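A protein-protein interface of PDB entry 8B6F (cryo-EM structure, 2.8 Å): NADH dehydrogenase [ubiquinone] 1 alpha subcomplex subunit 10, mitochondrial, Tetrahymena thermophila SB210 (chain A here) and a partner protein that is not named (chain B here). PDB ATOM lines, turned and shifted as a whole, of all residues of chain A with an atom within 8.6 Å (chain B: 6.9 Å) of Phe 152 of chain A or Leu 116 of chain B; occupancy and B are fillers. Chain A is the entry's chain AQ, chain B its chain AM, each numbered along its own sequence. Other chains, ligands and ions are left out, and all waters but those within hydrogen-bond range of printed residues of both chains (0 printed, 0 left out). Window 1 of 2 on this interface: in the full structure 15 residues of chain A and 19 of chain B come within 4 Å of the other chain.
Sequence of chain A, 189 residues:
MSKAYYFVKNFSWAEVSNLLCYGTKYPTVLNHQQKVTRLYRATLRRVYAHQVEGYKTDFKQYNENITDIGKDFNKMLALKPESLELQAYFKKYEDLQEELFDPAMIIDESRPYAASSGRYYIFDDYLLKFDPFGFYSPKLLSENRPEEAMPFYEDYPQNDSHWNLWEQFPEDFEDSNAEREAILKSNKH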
ATOM      1  N   LEU A 140      17.292  29.752  25.444  1.00  0.00           N
ATOM      2  CA  LEU A 140      17.783  28.635  24.652  1.00  0.00           C
ATOM      3  C   LEU A 140      18.476  27.610  25.538  1.00  0.00           C
ATOM      4  O   LEU A 140      19.138  27.961  26.517  1.00  0.00           O
ATOM      5  CB  LEU A 140      18.758  29.136  23.587  1.00  0.00           C
ATOM      6  CG  LEU A 140      18.165  29.944  22.437  1.00  0.00           C
ATOM      7  CD1 LEU A 140      19.264  30.669  21.692  1.00  0.00           C
ATOM      8  CD2 LEU A 140      17.397  29.037  21.497  1.00  0.00           C
ATOM      9  N   LEU A 141      18.326  26.330  25.187  1.00  0.00           N
ATOM     10  CA  LEU A 141      19.112  25.302  25.861  1.00  0.00           C
ATOM     11  C   LEU A 141      20.598  25.541  25.643  1.00  0.00           C
ATOM     12  O   LEU A 141      21.399  25.419  26.577  1.00  0.00           O
ATOM     13  CB  LEU A 141      18.708  23.912  25.370  1.00  0.00           C
ATOM     14  CG  LEU A 141      17.271  23.466  25.660  1.00  0.00           C
ATOM     15  CD1 LEU A 141      17.084  22.008  25.278  1.00  0.00           C
ATOM     16  CD2 LEU A 141      16.893  23.679  27.115  1.00  0.00           C
ATOM     17  N   SER A 142      20.987  25.879  24.416  1.00  0.00           N
ATOM     18  CA  SER A 142      22.298  26.464  24.172  1.00  0.00           C
ATOM     19  C   SER A 142      22.264  27.900  24.674  1.00  0.00           C
ATOM     20  O   SER A 142      21.591  28.753  24.090  1.00  0.00           O
ATOM     21  CB  SER A 142      22.650  26.399  22.689  1.00  0.00           C
ATOM     22  OG  SER A 142      21.693  27.088  21.904  1.00  0.00           O
ATOM     23  N   GLU A 143      22.995  28.171  25.757  1.00  0.00           N
ATOM     24  CA  GLU A 143      22.772  29.395  26.519  1.00  0.00           C
ATOM     25  C   GLU A 143      22.782  30.633  25.633  1.00  0.00           C
ATOM     26  O   GLU A 143      21.957  31.537  25.807  1.00  0.00           O
ATOM     27  CB  GLU A 143      23.830  29.521  27.616  1.00  0.00           C
ATOM     28  CG  GLU A 143      23.783  28.404  28.644  1.00  0.00           C
ATOM     29  CD  GLU A 143      24.780  28.615  29.764  1.00  0.00           C
ATOM     30  OE1 GLU A 143      25.641  29.509  29.632  1.00  0.00           O
ATOM     31  OE2 GLU A 143      24.702  27.891  30.780  1.00  0.00           O
ATOM     32  N   ASN A 144      23.696  30.689  24.670  1.00  0.00           N
ATOM     33  CA  ASN A 144      23.893  31.875  23.850  1.00  0.00           C
ATOM     34  C   ASN A 144      23.957  31.483  22.382  1.00  0.00           C
ATOM     35  O   ASN A 144      24.040  30.304  22.030  1.00  0.00           O
ATOM     36  CB  ASN A 144      25.171  32.620  24.255  1.00  0.00           C
ATOM     37  CG  ASN A 144      26.394  31.723  24.243  1.00  0.00           C
ATOM     38  OD1 ASN A 144      27.145  31.689  23.270  1.00  0.00           O
ATOM     39  ND2 ASN A 144      26.599  30.988  25.331  1.00  0.00           N
ATOM     40  N   ARG A 145      23.906  32.500  21.522  1.00  0.00           N
ATOM     41  CA  ARG A 145      24.087  32.311  20.093  1.00  0.00           C
ATOM     42  C   ARG A 145      25.527  32.647  19.743  1.00  0.00           C
ATOM     43  O   ARG A 145      25.906  33.826  19.812  1.00  0.00           O
ATOM     44  CB  ARG A 145      23.130  33.200  19.303  1.00  0.00           C
ATOM     45  CG  ARG A 145      21.666  32.835  19.452  1.00  0.00           C
ATOM     46  CD  ARG A 145      21.374  31.454  18.899  1.00  0.00           C
ATOM     47  NE  ARG A 145      19.962  31.279  18.587  1.00  0.00           N
ATOM     48  CZ  ARG A 145      19.427  30.151  18.141  1.00  0.00           C
ATOM     49  NH1 ARG A 145      20.157  29.063  17.964  1.00  0.00           N
ATOM     50  NH2 ARG A 145      18.127  30.114  17.862  1.00  0.00           N
ATOM     51  N   PRO A 146      26.359  31.679  19.367  1.00  0.00           N
ATOM     52  CA  PRO A 146      27.759  32.001  19.072  1.00  0.00           C
ATOM     53  C   PRO A 146      27.869  32.948  17.888  1.00  0.00           C
ATOM     54  O   PRO A 146      27.110  32.858  16.922  1.00  0.00           O
ATOM     55  CB  PRO A 146      28.379  30.635  18.763  1.00  0.00           C
ATOM     56  CG  PRO A 146      27.240  29.820  18.270  1.00  0.00           C
ATOM     57  CD  PRO A 146      26.046  30.273  19.053  1.00  0.00           C
ATOM     58  N   GLU A 147      28.830  33.859  17.970  1.00  0.00           N
ATOM     59  CA  GLU A 147      29.118  34.781  16.886  1.00  0.00           C
ATOM     60  C   GLU A 147      30.343  34.307  16.119  1.00  0.00           C
ATOM     61  O   GLU A 147      31.228  33.649  16.671  1.00  0.00           O
ATOM     62  CB  GLU A 147      29.346  36.198  17.414  1.00  0.00           C
ATOM     63  CG  GLU A 147      30.581  36.350  18.288  1.00  0.00           C
ATOM     64  CD  GLU A 147      30.736  37.759  18.825  1.00  0.00           C
ATOM     65  OE1 GLU A 147      29.732  38.502  18.844  1.00  0.00           O
ATOM     66  OE2 GLU A 147      31.859  38.128  19.224  1.00  0.00           O
ATOM     67  N   ALA A 149      33.891  34.146  14.450  1.00  0.00           N
ATOM     68  CA  ALA A 149      35.205  34.543  14.945  1.00  0.00           C
ATOM     69  C   ALA A 149      35.319  34.432  16.458  1.00  0.00           C
ATOM     70  O   ALA A 149      36.217  35.035  17.051  1.00  0.00           O
ATOM     71  CB  ALA A 149      35.574  35.968  14.513  1.00  0.00           C
ATOM     72  N   MET A 150      34.432  33.683  17.105  1.00  0.00           N
ATOM     73  CA  MET A 150      34.503  33.439  18.535  1.00  0.00           C
ATOM     74  C   MET A 150      34.169  31.981  18.816  1.00  0.00           C
ATOM     75  O   MET A 150      33.360  31.380  18.098  1.00  0.00           O
ATOM     76  CB  MET A 150      33.530  34.335  19.318  1.00  0.00           C
ATOM     77  CG  MET A 150      33.974  35.779  19.440  1.00  0.00           C
ATOM     78  SD  MET A 150      35.487  35.982  20.402  1.00  0.00           S
ATOM     79  CE  MET A 150      34.972  35.377  22.005  1.00  0.00           C
ATOM     80  N   PRO A 151      34.770  31.388  19.845  1.00  0.00           N
ATOM     81  CA  PRO A 151      34.370  30.036  20.247  1.00  0.00           C
ATOM     82  C   PRO A 151      32.990  30.033  20.885  1.00  0.00           C
ATOM     83  O   PRO A 151      32.445  31.069  21.269  1.00  0.00           O
ATOM     84  CB  PRO A 151      35.448  29.621  21.257  1.00  0.00           C
ATOM     85  CG  PRO A 151      36.575  30.564  21.045  1.00  0.00           C
ATOM     86  CD  PRO A 151      35.960  31.842  20.584  1.00  0.00           C
ATOM     87  N   PHE A 152      32.423  28.836  20.988  1.00  0.00           N
ATOM     88  CA  PHE A 152      31.122  28.639  21.618  1.00  0.00           C
ATOM     89  C   PHE A 152      31.345  28.300  23.087  1.00  0.00           C
ATOM     90  O   PHE A 152      31.755  27.183  23.418  1.00  0.00           O
ATOM     91  CB  PHE A 152      30.342  27.537  20.907  1.00  0.00           C
ATOM     92  CG  PHE A 152      28.995  27.264  21.509  1.00  0.00           C
ATOM     93  CD1 PHE A 152      28.850  26.329  22.517  1.00  0.00           C
ATOM     94  CD2 PHE A 152      27.874  27.936  21.061  1.00  0.00           C
ATOM     95  CE1 PHE A 152      27.612  26.076  23.072  1.00  0.00           C
ATOM     96  CE2 PHE A 152      26.634  27.687  21.609  1.00  0.00           C
ATOM     97  CZ  PHE A 152      26.502  26.756  22.616  1.00  0.00           C
ATOM     98  N   TYR A 153      31.079  29.263  23.966  1.00  0.00           N
ATOM     99  CA  TYR A 153      31.221  29.081  25.402  1.00  0.00           C
ATOM    100  C   TYR A 153      29.895  29.343  26.098  1.00  0.00           C
ATOM    101  O   TYR A 153      29.099  30.182  25.666  1.00  0.00           O
ATOM    102  CB  TYR A 153      32.293  30.012  25.980  1.00  0.00           C
ATOM    103  CG  TYR A 153      33.707  29.544  25.745  1.00  0.00           C
ATOM    104  CD1 TYR A 153      34.165  28.355  26.295  1.00  0.00           C
ATOM    105  CD2 TYR A 153      34.594  30.302  24.994  1.00  0.00           C
ATOM    106  CE1 TYR A 153      35.459  27.926  26.091  1.00  0.00           C
ATOM    107  CE2 TYR A 153      35.891  29.882  24.785  1.00  0.00           C
ATOM    108  CZ  TYR A 153      36.316  28.693  25.337  1.00  0.00           C
ATOM    109  OH  TYR A 153      37.609  28.271  25.131  1.00  0.00           O
ATOM    110  N   GLU A 154      29.666  28.612  27.185  1.00  0.00           N
ATOM    111  CA  GLU A 154      28.473  28.820  27.992  1.00  0.00           C
ATOM    112  C   GLU A 154      28.531  30.178  28.680  1.00  0.00           C
ATOM    113  O   GLU A 154      29.599  30.638  29.094  1.00  0.00           O
ATOM    114  CB  GLU A 154      28.341  27.718  29.043  1.00  0.00           C
ATOM    115  CG  GLU A 154      28.417  26.307  28.488  1.00  0.00           C
ATOM    116  CD  GLU A 154      28.414  25.260  29.585  1.00  0.00           C
ATOM    117  OE1 GLU A 154      28.111  25.618  30.741  1.00  0.00           O
ATOM    118  OE2 GLU A 154      28.718  24.084  29.293  1.00  0.00           O
ATOM    119  N   ASP A 155      27.376  30.824  28.800  1.00  0.00           N
ATOM    120  CA  ASP A 155      27.300  32.067  29.548  1.00  0.00           C
ATOM    121  C   ASP A 155      27.561  31.811  31.028  1.00  0.00           C
ATOM    122  O   ASP A 155      27.216  30.759  31.570  1.00  0.00           O
ATOM    123  CB  ASP A 155      25.930  32.723  29.373  1.00  0.00           C
ATOM    124  CG  ASP A 155      25.716  33.264  27.975  1.00  0.00           C
ATOM    125  OD1 ASP A 155      26.707  33.666  27.330  1.00  0.00           O
ATOM    126  OD2 ASP A 155      24.553  33.291  27.520  1.00  0.00           O
ATOM    127  N   HIS B  94      36.663  13.432  25.569  1.00  0.00           N
ATOM    128  CA  HIS B  94      35.421  12.751  25.243  1.00  0.00           C
ATOM    129  C   HIS B  94      35.709  11.754  24.129  1.00  0.00           C
ATOM    130  O   HIS B  94      36.855  11.578  23.710  1.00  0.00           O
ATOM    131  CB  HIS B  94      34.326  13.749  24.846  1.00  0.00           C
ATOM    132  CG  HIS B  94      34.018  14.757  25.909  1.00  0.00           C
ATOM    133  ND1 HIS B  94      32.980  14.605  26.803  1.00  0.00           N
ATOM    134  CD2 HIS B  94      34.611  15.934  26.220  1.00  0.00           C
ATOM    135  CE1 HIS B  94      32.948  15.642  27.619  1.00  0.00           C
ATOM    136  NE2 HIS B  94      33.927  16.464  27.287  1.00  0.00           N
ATOM    137  N   VAL B 113      36.168  19.759  22.780  1.00  0.00           N
ATOM    138  CA  VAL B 113      36.293  20.718  23.873  1.00  0.00           C
ATOM    139  C   VAL B 113      35.846  20.088  25.183  1.00  0.00           C
ATOM    140  O   VAL B 113      35.244  19.008  25.195  1.00  0.00           O
ATOM    141  CB  VAL B 113      35.493  22.002  23.592  1.00  0.00           C
ATOM    142  CG1 VAL B 113      36.076  22.730  22.397  1.00  0.00           C
ATOM    143  CG2 VAL B 113      34.019  21.685  23.382  1.00  0.00           C
ATOM    144  N   ALA B 114      36.138  20.763  26.297  1.00  0.00           N
ATOM    145  CA  ALA B 114      35.841  20.198  27.610  1.00  0.00           C
ATOM    146  C   ALA B 114      34.339  20.071  27.838  1.00  0.00           C
ATOM    147  O   ALA B 114      33.852  19.002  28.226  1.00  0.00           O
ATOM    148  CB  ALA B 114      36.476  21.062  28.700  1.00  0.00           C
ATOM    149  N   THR B 115      33.586  21.145  27.608  1.00  0.00           N
ATOM    150  CA  THR B 115      32.155  21.128  27.876  1.00  0.00           C
ATOM    151  C   THR B 115      31.442  22.055  26.903  1.00  0.00           C
ATOM    152  O   THR B 115      32.041  22.964  26.326  1.00  0.00           O
ATOM    153  CB  THR B 115      31.832  21.547  29.317  1.00  0.00           C
ATOM    154  OG1 THR B 115      32.368  22.852  29.573  1.00  0.00           O
ATOM    155  CG2 THR B 115      32.406  20.554  30.322  1.00  0.00           C
ATOM    156  N   LEU B 116      30.144  21.809  26.739  1.00  0.00           N
ATOM    157  CA  LEU B 116      29.278  22.634  25.913  1.00  0.00           C
ATOM    158  C   LEU B 116      27.945  22.802  26.626  1.00  0.00           C
ATOM    159  O   LEU B 116      27.687  22.183  27.662  1.00  0.00           O
ATOM    160  CB  LEU B 116      29.070  22.022  24.521  1.00  0.00           C
ATOM    161  CG  LEU B 116      30.289  22.023  23.597  1.00  0.00           C
ATOM    162  CD1 LEU B 116      30.050  21.124  22.398  1.00  0.00           C
ATOM    163  CD2 LEU B 116      30.611  23.432  23.145  1.00  0.00           C
ATOM    164  N   ALA B 117      27.090  23.646  26.059  1.00  0.00           N
ATOM    165  CA  ALA B 117      25.801  23.931  26.666  1.00  0.00           C
ATOM    166  C   ALA B 117      24.916  22.684  26.630  1.00  0.00           C
ATOM    167  O   ALA B 117      25.295  21.627  26.119  1.00  0.00           O
ATOM    168  CB  ALA B 117      25.131  25.101  25.956  1.00  0.00           C
ATOM    169  N   ALA B 118      23.719  22.813  27.193  1.00  0.00           N
ATOM    170  CA  ALA B 118      22.814  21.678  27.298  1.00  0.00           C
ATOM    171  C   ALA B 118      22.302  21.257  25.926  1.00  0.00           C
ATOM    172  O   ALA B 118      22.011  22.093  25.068  1.00  0.00           O
ATOM    173  CB  ALA B 118      21.636  22.024  28.207  1.00  0.00           C
ATOM    174  N   GLY B 119      22.197  19.946  25.724  1.00  0.00           N
ATOM    175  CA  GLY B 119      21.662  19.396  24.498  1.00  0.00           C
ATOM    176  C   GLY B 119      22.656  19.256  23.369  1.00  0.00           C
ATOM    177  O   GLY B 119      22.297  18.708  22.319  1.00  0.00           O
ATOM    178  N   ILE B 120      23.884  19.724  23.544  1.00  0.00           N
ATOM    179  CA  ILE B 120      24.921  19.680  22.518  1.00  0.00           C
ATOM    180  C   ILE B 120      25.925  18.605  22.917  1.00  0.00           C
ATOM    181  O   ILE B 120      26.577  18.738  23.961  1.00  0.00           O
ATOM    182  CB  ILE B 120      25.615  21.042  22.356  1.00  0.00           C
ATOM    183  CG1 ILE B 120      24.577  22.132  22.076  1.00  0.00           C
ATOM    184  CG2 ILE B 120      26.655  20.972  21.240  1.00  0.00           C
ATOM    185  CD1 ILE B 120      25.158  23.519  21.891  1.00  0.00           C
ATOM    186  N   PRO B 121      26.082  17.531  22.143  1.00  0.00           N
ATOM    187  CA  PRO B 121      27.095  16.530  22.493  1.00  0.00           C
ATOM    188  C   PRO B 121      28.495  17.124  22.440  1.00  0.00           C
ATOM    189  O   PRO B 121      28.803  17.963  21.593  1.00  0.00           O
ATOM    190  CB  PRO B 121      26.896  15.436  21.438  1.00  0.00           C
ATOM    191  CG  PRO B 121      26.256  16.124  20.295  1.00  0.00           C
ATOM    192  CD  PRO B 121      25.392  17.192  20.887  1.00  0.00           C
ATOM    193  N   VAL B 122      29.345  16.668  23.353  1.00  0.00           N
ATOM    194  CA  VAL B 122      30.724  17.132  23.435  1.00  0.00           C
ATOM    195  C   VAL B 122      31.681  16.125  22.795  1.00  0.00           C
ATOM    196  O   VAL B 122      32.868  16.103  23.116  1.00  0.00           O
ATOM    197  CB  VAL B 122      31.126  17.439  24.887  1.00  0.00           C
ATOM    198  CG1 VAL B 122      32.368  18.317  24.930  1.00  0.00           C
ATOM    199  CG2 VAL B 122      29.980  18.108  25.633  1.00  0.00           C
ATOM    200  N   SER B 123      31.177  15.288  21.896  1.00  0.00           N
ATOM    201  CA  SER B 123      31.968  14.292  21.199  1.00  0.00           C
ATOM    202  C   SER B 123      31.818  14.477  19.697  1.00  0.00           C
ATOM    203  O   SER B 123      30.803  14.989  19.218  1.00  0.00           O
ATOM    204  CB  SER B 123      31.527  12.885  21.592  1.00  0.00           C
ATOM    205  OG  SER B 123      30.159  12.704  21.273  1.00  0.00           O
ATOM    206  N   GLN B 139      36.234  19.882  15.841  1.00  0.00           N
ATOM    207  CA  GLN B 139      36.039  19.954  17.286  1.00  0.00           C
ATOM    208  C   GLN B 139      34.558  19.800  17.600  1.00  0.00           C
ATOM    209  O   GLN B 139      33.753  20.660  17.231  1.00  0.00           O
ATOM    210  CB  GLN B 139      36.580  21.267  17.846  1.00  0.00           C
ATOM    211  CG  GLN B 139      38.061  21.469  17.597  1.00  0.00           C
ATOM    212  CD  GLN B 139      38.653  22.535  18.488  1.00  0.00           C
ATOM    213  OE1 GLN B 139      37.933  23.238  19.197  1.00  0.00           O
ATOM    214  NE2 GLN B 139      39.975  22.662  18.461  1.00  0.00           N
ATOM    215  N   SER B 140      34.207  18.712  18.281  1.00  0.00           N
ATOM    216  CA  SER B 140      32.864  18.492  18.817  1.00  0.00           C
ATOM    217  C   SER B 140      31.786  18.847  17.798  1.00  0.00           C
ATOM    218  O   SER B 140      30.854  19.604  18.073  1.00  0.00           O
ATOM    219  CB  SER B 140      32.665  19.285  20.107  1.00  0.00           C
ATOM    220  OG  SER B 140      33.597  18.886  21.094  1.00  0.00           O
ATOM    221  N   CYS B 141      31.917  18.276  16.606  1.00  0.00           N
ATOM    222  CA  CYS B 141      31.012  18.549  15.501  1.00  0.00           C
ATOM    223  C   CYS B 141      30.313  17.267  15.076  1.00  0.00           C
ATOM    224  O   CYS B 141      30.868  16.171  15.186  1.00  0.00           O
ATOM    225  CB  CYS B 141      31.762  19.150  14.311  1.00  0.00           C
ATOM    226  SG  CYS B 141      33.089  18.107  13.685  1.00  0.00           S
ATOM    227  N   LEU B 156      34.076  23.881  14.038  1.00  0.00           N
ATOM    228  CA  LEU B 156      34.157  24.188  15.456  1.00  0.00           C
ATOM    229  C   LEU B 156      33.035  23.493  16.225  1.00  0.00           C
ATOM    230  O   LEU B 156      32.293  22.667  15.688  1.00  0.00           O
ATOM    231  CB  LEU B 156      34.127  25.705  15.652  1.00  0.00           C
ATOM    232  CG  LEU B 156      35.219  26.489  14.921  1.00  0.00           C
ATOM    233  CD1 LEU B 156      35.112  27.972  15.239  1.00  0.00           C
ATOM    234  CD2 LEU B 156      36.604  25.967  15.269  1.00  0.00           C
ATOM    235  N   GLU B 157      32.913  23.834  17.506  1.00  0.00           N
ATOM    236  CA  GLU B 157      32.011  23.127  18.403  1.00  0.00           C
ATOM    237  C   GLU B 157      30.551  23.352  18.026  1.00  0.00           C
ATOM    238  O   GLU B 157      30.174  24.403  17.503  1.00  0.00           O
ATOM    239  CB  GLU B 157      32.229  23.580  19.844  1.00  0.00           C
ATOM    240  CG  GLU B 157      33.667  23.527  20.309  1.00  0.00           C
ATOM    241  CD  GLU B 157      34.440  24.796  20.001  1.00  0.00           C
ATOM    242  OE1 GLU B 157      33.847  25.891  20.073  1.00  0.00           O
ATOM    243  OE2 GLU B 157      35.643  24.698  19.681  1.00  0.00           O
ATOM    244  N   GLY B 158      29.729  22.345  18.304  1.00  0.00           N
ATOM    245  CA  GLY B 158      28.294  22.455  18.132  1.00  0.00           C
ATOM    246  C   GLY B 158      27.828  22.636  16.710  1.00  0.00           C
ATOM    247  O   GLY B 158      26.658  22.962  16.496  1.00  0.00           O
ATOM    248  N   ALA B 175      31.323  27.904  15.103  1.00  0.00           N
ATOM    249  CA  ALA B 175      30.780  27.022  16.125  1.00  0.00           C
ATOM    250  C   ALA B 175      29.274  27.209  16.255  1.00  0.00           C
ATOM    251  O   ALA B 175      28.752  28.319  16.122  1.00  0.00           O
ATOM    252  CB  ALA B 175      31.457  27.292  17.467  1.00  0.00           C
ATOM    253  N   GLY B 176      28.571  26.107  16.508  1.00  0.00           N
ATOM    254  CA  GLY B 176      27.144  26.158  16.747  1.00  0.00           C
ATOM    255  C   GLY B 176      26.319  26.615  15.563  1.00  0.00           C
ATOM    256  O   GLY B 176      25.419  27.445  15.722  1.00  0.00           O
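Printed residues of chain A that touch a printed residue of chain B: Leu 141, Ser 142, Glu 143, Pro 146, Phe 152 and Glu 154. Hydrophobic or aromatic side chains of chain A that line the printed part of chain B: Leu 141, Pro 146 and Phe 152. Along chain A the printed residues that touch a printed residue of chain B span positions 141 to 154. Among the printed residues, 16 pairs touch across the chains.
O of Leu 116 of chain B lies close to OE2 of Glu 154 of chain A (2.7 Å). The side-chain carboxylate (OE1) of Glu 157 of chain B sits at hydrogen-bond distance from the backbone NH (N) of Phe 152 of chain A (3.4 Å).
O of Leu 141 of chain A touches CB of Ala 117 of chain B, 3.8 Å away. Leu 141 of chain A touches Ala 118 of chain B. Ser 142 of chain A touches Ala 117 of chain B. N of Ser 142 of chain A touches O of Ala 118 of chain B, at 3.98 Å. Ser 142 of chain A touches Ile 120 of chain B. Phe 152 of chain A touches Leu 116 of chain B. Phe 152 of chain A touches Ala 117 of chain B. Ala 175 of chain B touches Phe 152 of chain A. OE2 of Glu 154 of chain A touches OG1 of Thr 115 of chain B, at 3.9 Å. Glu 154 of chain A touches Ala 117 of chain B (OE2 to N, 3.6 Å).
Of chain B, only Leu 116, Ala 117, Ile 120, Glu 157 and Ala 175 come within 4 Å of Phe 152 of chain A. Leu 116 of chain B touches just these residues of chain A: Phe 152 (3.4 Å) and Glu 154 (2.7 Å). Of chain A, only Leu 141 (3.8 Å), Ser 142 (3.6 Å), Glu 143 (3.7 Å), Phe 152 (3.9 Å) and Glu 154 (3.6 Å) come within 4 Å of Ala 117 of chain B. Of the printed residues of chain B, Glu 154 of chain A touches Thr 115 (3.9 Å), Leu 116 (2.7 Å) and Ala 117 (3.6 Å). Of the printed residues of chain A, Ala 118 of chain B touches Leu 141 (3.5 Å) and Ser 142 (3.98 Å). Of the printed residues of chain B, Pro 146 of chain A touches Ala 175 and Gly 176. Printed residues of chain A within 4 Å of Gly 176 of chain B: Pro 146. The nearest residue of chain A that does not touch Leu 116 of chain B is Tyr 153 of chain A (5.9 Å). The nearest printed residue of chain B that does not touch Pro 146 of chain A is Glu 157 of chain B (6.2 Å).
The side-chain amide oxygen of Gln 139 of chain B lies close to the side-chain carboxylate of Glu 157 of chain B (2.8 Å). O of Glu 157 of chain B sits at hydrogen-bond distance from N of Gly 176 of chain B (2.5 Å).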
